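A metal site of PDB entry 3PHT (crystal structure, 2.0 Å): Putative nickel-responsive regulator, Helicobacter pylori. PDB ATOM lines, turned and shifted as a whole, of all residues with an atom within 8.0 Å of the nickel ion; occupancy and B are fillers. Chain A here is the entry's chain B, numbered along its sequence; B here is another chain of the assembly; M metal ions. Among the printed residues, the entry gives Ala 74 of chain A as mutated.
A ring nitrogen (ND1) of His 99 sits at hydrogen-bond distance from the side-chain carboxylate (OE1) of Glu 109 (2.6 Å). O of Asp 103 lies within hydrogen-bond range of ND1 of His 88 of chain B (2.8 Å). N of His 99 is in hydrogen-bond range of O of Thr 97 of chain B (2.9 Å). OE1 of Gln 87 of chain B is in hydrogen-bond range of NE2 of His 101, 2.8 Å away. The backbone NH of Cys 107 lies within hydrogen-bond range of the backbone carbonyl oxygen of Tyr 72 (2.9 Å). ND1 of His 99 lies close to OH of Tyr 72, at 3.3 Å.
Of the 22 residues printed, 4 come within 4 Å of the nickel ion. The nearest printed residue that does not touch the nickel ion is Ile 100 (4.1 Å).
The nickel ion is bound by ND1 of His 101 (2.0 Å). NE2 of His 99 binds the nickel ion (2.1 Å). The nickel ion is bound by NE2 of His 88 of chain B (2.1 Å). The nickel ion is bound by the side-chain sulfur (SG) of Cys 107, at 2.2 Å. The nickel ion has four donor atoms within binding distance.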
ATOM      1  N   TYR A  72     -12.395  17.724 -15.964  1.00  0.00           N
ATOM      2  CA  TYR A  72     -11.655  16.745 -15.229  1.00  0.00           C
ATOM      3  C   TYR A  72     -10.467  16.244 -15.982  1.00  0.00           C
ATOM      4  O   TYR A  72     -10.351  16.358 -17.235  1.00  0.00           O
ATOM      5  CB  TYR A  72     -12.520  15.558 -14.755  1.00  0.00           C
ATOM      6  CG  TYR A  72     -13.206  14.708 -15.832  1.00  0.00           C
ATOM      7  CD1 TYR A  72     -12.569  13.590 -16.354  1.00  0.00           C
ATOM      8  CD2 TYR A  72     -14.487  15.008 -16.283  1.00  0.00           C
ATOM      9  CE1 TYR A  72     -13.156  12.797 -17.301  1.00  0.00           C
ATOM     10  CE2 TYR A  72     -15.104  14.216 -17.235  1.00  0.00           C
ATOM     11  CZ  TYR A  72     -14.423  13.122 -17.738  1.00  0.00           C
ATOM     12  OH  TYR A  72     -14.998  12.302 -18.674  1.00  0.00           O
ATOM     13  N   ASP A  73      -9.578  15.688 -15.189  1.00  0.00           N
ATOM     14  CA  ASP A  73      -8.314  15.152 -15.691  1.00  0.00           C
ATOM     15  C   ASP A  73      -8.589  13.871 -16.506  1.00  0.00           C
ATOM     16  O   ASP A  73      -8.960  12.821 -15.946  1.00  0.00           O
ATOM     17  CB  ASP A  73      -7.404  14.891 -14.514  1.00  0.00           C
ATOM     18  CG  ASP A  73      -6.092  14.156 -14.883  1.00  0.00           C
ATOM     19  OD1 ASP A  73      -5.808  13.793 -16.079  1.00  0.00           O
ATOM     20  OD2 ASP A  73      -5.344  13.940 -13.911  1.00  0.00           O
ATOM     21  N   ALA A  74      -8.359  13.979 -17.813  1.00  0.00           N
ATOM     22  CA  ALA A  74      -8.482  12.873 -18.780  1.00  0.00           C
ATOM     23  C   ALA A  74      -7.544  11.643 -18.509  1.00  0.00           C
ATOM     24  O   ALA A  74      -7.511  10.713 -19.319  1.00  0.00           O
ATOM     25  CB  ALA A  74      -8.216  13.423 -20.182  1.00  0.00           C
ATOM     26  N   ASN A  80     -13.444   8.352 -14.413  1.00  0.00           N
ATOM     27  CA  ASN A  80     -14.678   8.361 -15.225  1.00  0.00           C
ATOM     28  C   ASN A  80     -15.528   7.114 -14.949  1.00  0.00           C
ATOM     29  O   ASN A  80     -16.722   7.328 -14.927  1.00  0.00           O
ATOM     30  CB  ASN A  80     -14.565   8.725 -16.758  1.00  0.00           C
ATOM     31  CG  ASN A  80     -15.920   9.237 -17.357  1.00  0.00           C
ATOM     32  OD1 ASN A  80     -16.726   9.890 -16.658  1.00  0.00           O
ATOM     33  ND2 ASN A  80     -16.168   8.916 -18.616  1.00  0.00           N
ATOM     34  N   HIS A  99     -19.568  15.350 -24.058  1.00  0.00           N
ATOM     35  CA  HIS A  99     -18.191  15.371 -23.601  1.00  0.00           C
ATOM     36  C   HIS A  99     -17.369  15.922 -24.754  1.00  0.00           C
ATOM     37  O   HIS A  99     -17.551  15.554 -25.901  1.00  0.00           O
ATOM     38  CB  HIS A  99     -17.786  13.899 -23.404  1.00  0.00           C
ATOM     39  CG  HIS A  99     -16.399  13.711 -22.911  1.00  0.00           C
ATOM     40  ND1 HIS A  99     -16.133  13.212 -21.648  1.00  0.00           N
ATOM     41  CD2 HIS A  99     -15.192  13.957 -23.509  1.00  0.00           C
ATOM     42  CE1 HIS A  99     -14.817  13.082 -21.511  1.00  0.00           C
ATOM     43  NE2 HIS A  99     -14.239  13.574 -22.593  1.00  0.00           N
ATOM     44  N   ILE A 100     -16.540  16.886 -24.425  1.00  0.00           N
ATOM     45  CA  ILE A 100     -15.512  17.421 -25.322  1.00  0.00           C
ATOM     46  C   ILE A 100     -14.126  17.069 -24.819  1.00  0.00           C
ATOM     47  O   ILE A 100     -13.802  17.340 -23.626  1.00  0.00           O
ATOM     48  CB  ILE A 100     -15.621  18.998 -25.298  1.00  0.00           C
ATOM     49  CG1 ILE A 100     -17.008  19.422 -25.759  1.00  0.00           C
ATOM     50  CG2 ILE A 100     -14.435  19.629 -26.111  1.00  0.00           C
ATOM     51  CD1 ILE A 100     -17.205  19.082 -27.296  1.00  0.00           C
ATOM     52  N   HIS A 101     -13.287  16.499 -25.690  1.00  0.00           N
ATOM     53  CA  HIS A 101     -11.917  16.190 -25.306  1.00  0.00           C
ATOM     54  C   HIS A 101     -11.094  17.480 -25.548  1.00  0.00           C
ATOM     55  O   HIS A 101     -10.748  17.792 -26.667  1.00  0.00           O
ATOM     56  CB  HIS A 101     -11.347  14.989 -26.129  1.00  0.00           C
ATOM     57  CG  HIS A 101     -12.277  13.806 -26.146  1.00  0.00           C
ATOM     58  ND1 HIS A 101     -12.692  13.140 -25.002  1.00  0.00           N
ATOM     59  CD2 HIS A 101     -12.887  13.168 -27.194  1.00  0.00           C
ATOM     60  CE1 HIS A 101     -13.536  12.152 -25.345  1.00  0.00           C
ATOM     61  NE2 HIS A 101     -13.685  12.177 -26.657  1.00  0.00           N
ATOM     62  N   MET A 102     -10.832  18.265 -24.502  1.00  0.00           N
ATOM     63  CA  MET A 102     -10.312  19.631 -24.732  1.00  0.00           C
ATOM     64  C   MET A 102      -8.857  19.573 -25.109  1.00  0.00           C
ATOM     65  O   MET A 102      -8.454  20.314 -25.966  1.00  0.00           O
ATOM     66  CB  MET A 102     -10.404  20.524 -23.512  1.00  0.00           C
ATOM     67  CG  MET A 102     -11.830  20.865 -23.007  1.00  0.00           C
ATOM     68  SD  MET A 102     -11.794  21.260 -21.233  1.00  0.00           S
ATOM     69  CE  MET A 102     -10.909  22.797 -21.106  1.00  0.00           C
ATOM     70  N   ASP A 103      -8.050  18.750 -24.417  1.00  0.00           N
ATOM     71  CA  ASP A 103      -6.612  18.552 -24.774  1.00  0.00           C
ATOM     72  C   ASP A 103      -6.185  17.268 -24.102  1.00  0.00           C
ATOM     73  O   ASP A 103      -7.030  16.568 -23.523  1.00  0.00           O
ATOM     74  CB  ASP A 103      -5.710  19.714 -24.300  1.00  0.00           C
ATOM     75  CG  ASP A 103      -5.918  20.062 -22.823  1.00  0.00           C
ATOM     76  OD1 ASP A 103      -5.931  19.174 -21.954  1.00  0.00           O
ATOM     77  OD2 ASP A 103      -6.103  21.254 -22.520  1.00  0.00           O
ATOM     78  N   GLU A 104      -4.897  16.986 -24.130  1.00  0.00           N
ATOM     79  CA  GLU A 104      -4.406  15.691 -23.698  1.00  0.00           C
ATOM     80  C   GLU A 104      -4.718  15.427 -22.241  1.00  0.00           C
ATOM     81  O   GLU A 104      -4.851  14.279 -21.859  1.00  0.00           O
ATOM     82  CB  GLU A 104      -2.896  15.534 -23.981  1.00  0.00           C
ATOM     83  CG  GLU A 104      -2.407  14.087 -24.020  1.00  0.00           C
ATOM     84  CD  GLU A 104      -0.889  13.974 -24.182  1.00  0.00           C
ATOM     85  OE1 GLU A 104      -0.337  14.612 -25.103  1.00  0.00           O
ATOM     86  OE2 GLU A 104      -0.253  13.214 -23.408  1.00  0.00           O
ATOM     87  N   HIS A 105      -4.860  16.482 -21.433  1.00  0.00           N
ATOM     88  CA  HIS A 105      -5.093  16.286 -19.983  1.00  0.00           C
ATOM     89  C   HIS A 105      -6.461  16.684 -19.426  1.00  0.00           C
ATOM     90  O   HIS A 105      -6.637  16.631 -18.205  1.00  0.00           O
ATOM     91  CB  HIS A 105      -4.016  17.021 -19.186  1.00  0.00           C
ATOM     92  CG  HIS A 105      -2.614  16.743 -19.635  1.00  0.00           C
ATOM     93  ND1 HIS A 105      -1.865  15.691 -19.132  1.00  0.00           N
ATOM     94  CD2 HIS A 105      -1.817  17.387 -20.524  1.00  0.00           C
ATOM     95  CE1 HIS A 105      -0.674  15.699 -19.702  1.00  0.00           C
ATOM     96  NE2 HIS A 105      -0.616  16.718 -20.552  1.00  0.00           N
ATOM     97  N   ASN A 106      -7.406  17.124 -20.270  1.00  0.00           N
ATOM     98  CA  ASN A 106      -8.683  17.678 -19.789  1.00  0.00           C
ATOM     99  C   ASN A 106      -9.845  17.283 -20.665  1.00  0.00           C
ATOM    100  O   ASN A 106      -9.750  17.326 -21.880  1.00  0.00           O
ATOM    101  CB  ASN A 106      -8.658  19.231 -19.716  1.00  0.00           C
ATOM    102  CG  ASN A 106      -7.593  19.781 -18.681  1.00  0.00           C
ATOM    103  OD1 ASN A 106      -7.867  19.872 -17.471  1.00  0.00           O
ATOM    104  ND2 ASN A 106      -6.410  20.115 -19.162  1.00  0.00           N
ATOM    105  N   CYS A 107     -10.921  16.888 -19.993  1.00  0.00           N
ATOM    106  CA  CYS A 107     -12.177  16.611 -20.564  1.00  0.00           C
ATOM    107  C   CYS A 107     -13.167  17.569 -19.997  1.00  0.00           C
ATOM    108  O   CYS A 107     -13.082  17.908 -18.825  1.00  0.00           O
ATOM    109  CB  CYS A 107     -12.618  15.206 -20.184  1.00  0.00           C
ATOM    110  SG  CYS A 107     -11.561  13.907 -20.990  1.00  0.00           S
ATOM    111  N   LEU A 108     -14.121  17.998 -20.820  1.00  0.00           N
ATOM    112  CA  LEU A 108     -15.217  18.809 -20.322  1.00  0.00           C
ATOM    113  C   LEU A 108     -16.499  18.016 -20.540  1.00  0.00           C
ATOM    114  O   LEU A 108     -16.666  17.410 -21.608  1.00  0.00           O
ATOM    115  CB  LEU A 108     -15.353  20.136 -21.060  1.00  0.00           C
ATOM    116  CG  LEU A 108     -16.763  20.819 -20.947  1.00  0.00           C
ATOM    117  CD1 LEU A 108     -16.796  21.711 -19.765  1.00  0.00           C
ATOM    118  CD2 LEU A 108     -17.037  21.692 -22.210  1.00  0.00           C
ATOM    119  N   GLU A 109     -17.380  18.002 -19.526  1.00  0.00           N
ATOM    120  CA  GLU A 109     -18.698  17.357 -19.769  1.00  0.00           C
ATOM    121  C   GLU A 109     -19.813  18.260 -19.357  1.00  0.00           C
ATOM    122  O   GLU A 109     -19.649  18.968 -18.357  1.00  0.00           O
ATOM    123  CB  GLU A 109     -18.840  16.049 -18.937  1.00  0.00           C
ATOM    124  CG  GLU A 109     -18.120  14.962 -19.662  1.00  0.00           C
ATOM    125  CD  GLU A 109     -18.305  13.557 -19.049  1.00  0.00           C
ATOM    126  OE1 GLU A 109     -17.627  12.615 -19.550  1.00  0.00           O
ATOM    127  OE2 GLU A 109     -19.083  13.371 -18.096  1.00  0.00           O
ATOM    128  N   MET B  83     -11.399   4.088 -23.704  1.00  0.00           N
ATOM    129  CA  MET B  83     -12.109   4.782 -24.765  1.00  0.00           C
ATOM    130  C   MET B  83     -11.726   6.279 -24.817  1.00  0.00           C
ATOM    131  O   MET B  83     -11.586   6.817 -25.881  1.00  0.00           O
ATOM    132  CB  MET B  83     -13.627   4.647 -24.541  1.00  0.00           C
ATOM    133  CG  MET B  83     -14.162   3.285 -25.141  1.00  0.00           C
ATOM    134  SD  MET B  83     -15.900   3.093 -24.721  1.00  0.00           S
ATOM    135  CE  MET B  83     -16.572   4.137 -26.061  1.00  0.00           C
ATOM    136  N   ILE B  84     -11.611   6.919 -23.646  1.00  0.00           N
ATOM    137  CA  ILE B  84     -11.172   8.320 -23.512  1.00  0.00           C
ATOM    138  C   ILE B  84      -9.751   8.470 -24.051  1.00  0.00           C
ATOM    139  O   ILE B  84      -9.439   9.345 -24.902  1.00  0.00           O
ATOM    140  CB  ILE B  84     -11.154   8.727 -21.989  1.00  0.00           C
ATOM    141  CG1 ILE B  84     -12.557   9.025 -21.510  1.00  0.00           C
ATOM    142  CG2 ILE B  84     -10.142   9.869 -21.718  1.00  0.00           C
ATOM    143  CD1 ILE B  84     -13.557   9.421 -22.635  1.00  0.00           C
ATOM    144  N   ASP B  85      -8.865   7.599 -23.561  1.00  0.00           N
ATOM    145  CA  ASP B  85      -7.478   7.626 -24.034  1.00  0.00           C
ATOM    146  C   ASP B  85      -7.453   7.549 -25.557  1.00  0.00           C
ATOM    147  O   ASP B  85      -6.736   8.293 -26.233  1.00  0.00           O
ATOM    148  CB  ASP B  85      -6.624   6.437 -23.518  1.00  0.00           C
ATOM    149  CG  ASP B  85      -6.390   6.448 -21.999  1.00  0.00           C
ATOM    150  OD1 ASP B  85      -6.606   7.494 -21.329  1.00  0.00           O
ATOM    151  OD2 ASP B  85      -5.986   5.373 -21.484  1.00  0.00           O
ATOM    152  N   GLN B  87      -9.791   8.271 -27.737  1.00  0.00           N
ATOM    153  CA  GLN B  87     -10.315   9.459 -28.393  1.00  0.00           C
ATOM    154  C   GLN B  87      -9.381  10.687 -28.293  1.00  0.00           C
ATOM    155  O   GLN B  87      -9.250  11.452 -29.259  1.00  0.00           O
ATOM    156  CB  GLN B  87     -11.704   9.780 -27.831  1.00  0.00           C
ATOM    157  CG  GLN B  87     -12.750   8.812 -28.406  1.00  0.00           C
ATOM    158  CD  GLN B  87     -13.992   8.890 -27.618  1.00  0.00           C
ATOM    159  OE1 GLN B  87     -14.740   9.851 -27.760  1.00  0.00           O
ATOM    160  NE2 GLN B  87     -14.123   8.012 -26.639  1.00  0.00           N
ATOM    161  N   HIS B  88      -8.739  10.858 -27.122  1.00  0.00           N
ATOM    162  CA  HIS B  88      -7.800  11.972 -26.859  1.00  0.00           C
ATOM    163  C   HIS B  88      -6.536  11.865 -27.722  1.00  0.00           C
ATOM    164  O   HIS B  88      -6.012  12.912 -28.159  1.00  0.00           O
ATOM    165  CB  HIS B  88      -7.404  12.051 -25.374  1.00  0.00           C
ATOM    166  CG  HIS B  88      -8.385  12.799 -24.542  1.00  0.00           C
ATOM    167  ND1 HIS B  88      -8.113  14.047 -24.019  1.00  0.00           N
ATOM    168  CD2 HIS B  88      -9.659  12.509 -24.185  1.00  0.00           C
ATOM    169  CE1 HIS B  88      -9.176  14.494 -23.385  1.00  0.00           C
ATOM    170  NE2 HIS B  88     -10.110  13.587 -23.459  1.00  0.00           N
ATOM    171  N   VAL B  94     -12.160  13.919 -33.167  1.00  0.00           N
ATOM    172  CA  VAL B  94     -13.410  13.571 -32.388  1.00  0.00           C
ATOM    173  C   VAL B  94     -14.049  14.873 -31.996  1.00  0.00           C
ATOM    174  O   VAL B  94     -13.466  15.572 -31.203  1.00  0.00           O
ATOM    175  CB  VAL B  94     -13.102  12.758 -31.108  1.00  0.00           C
ATOM    176  CG1 VAL B  94     -14.412  12.511 -30.299  1.00  0.00           C
ATOM    177  CG2 VAL B  94     -12.415  11.388 -31.507  1.00  0.00           C
ATOM    178  N   THR B  97     -18.894  13.619 -27.924  1.00  0.00           N
ATOM    179  CA  THR B  97     -19.596  12.356 -27.672  1.00  0.00           C
ATOM    180  C   THR B  97     -20.796  12.631 -26.787  1.00  0.00           C
ATOM    181  O   THR B  97     -20.737  13.376 -25.837  1.00  0.00           O
ATOM    182  CB  THR B  97     -18.772  11.330 -26.942  1.00  0.00           C
ATOM    183  OG1 THR B  97     -18.783  11.671 -25.546  1.00  0.00           O
ATOM    184  CG2 THR B  97     -17.309  11.226 -27.488  1.00  0.00           C
HETATM  185 NI    NI M   1     -12.190  13.562 -23.088  1.00  0.00          NI
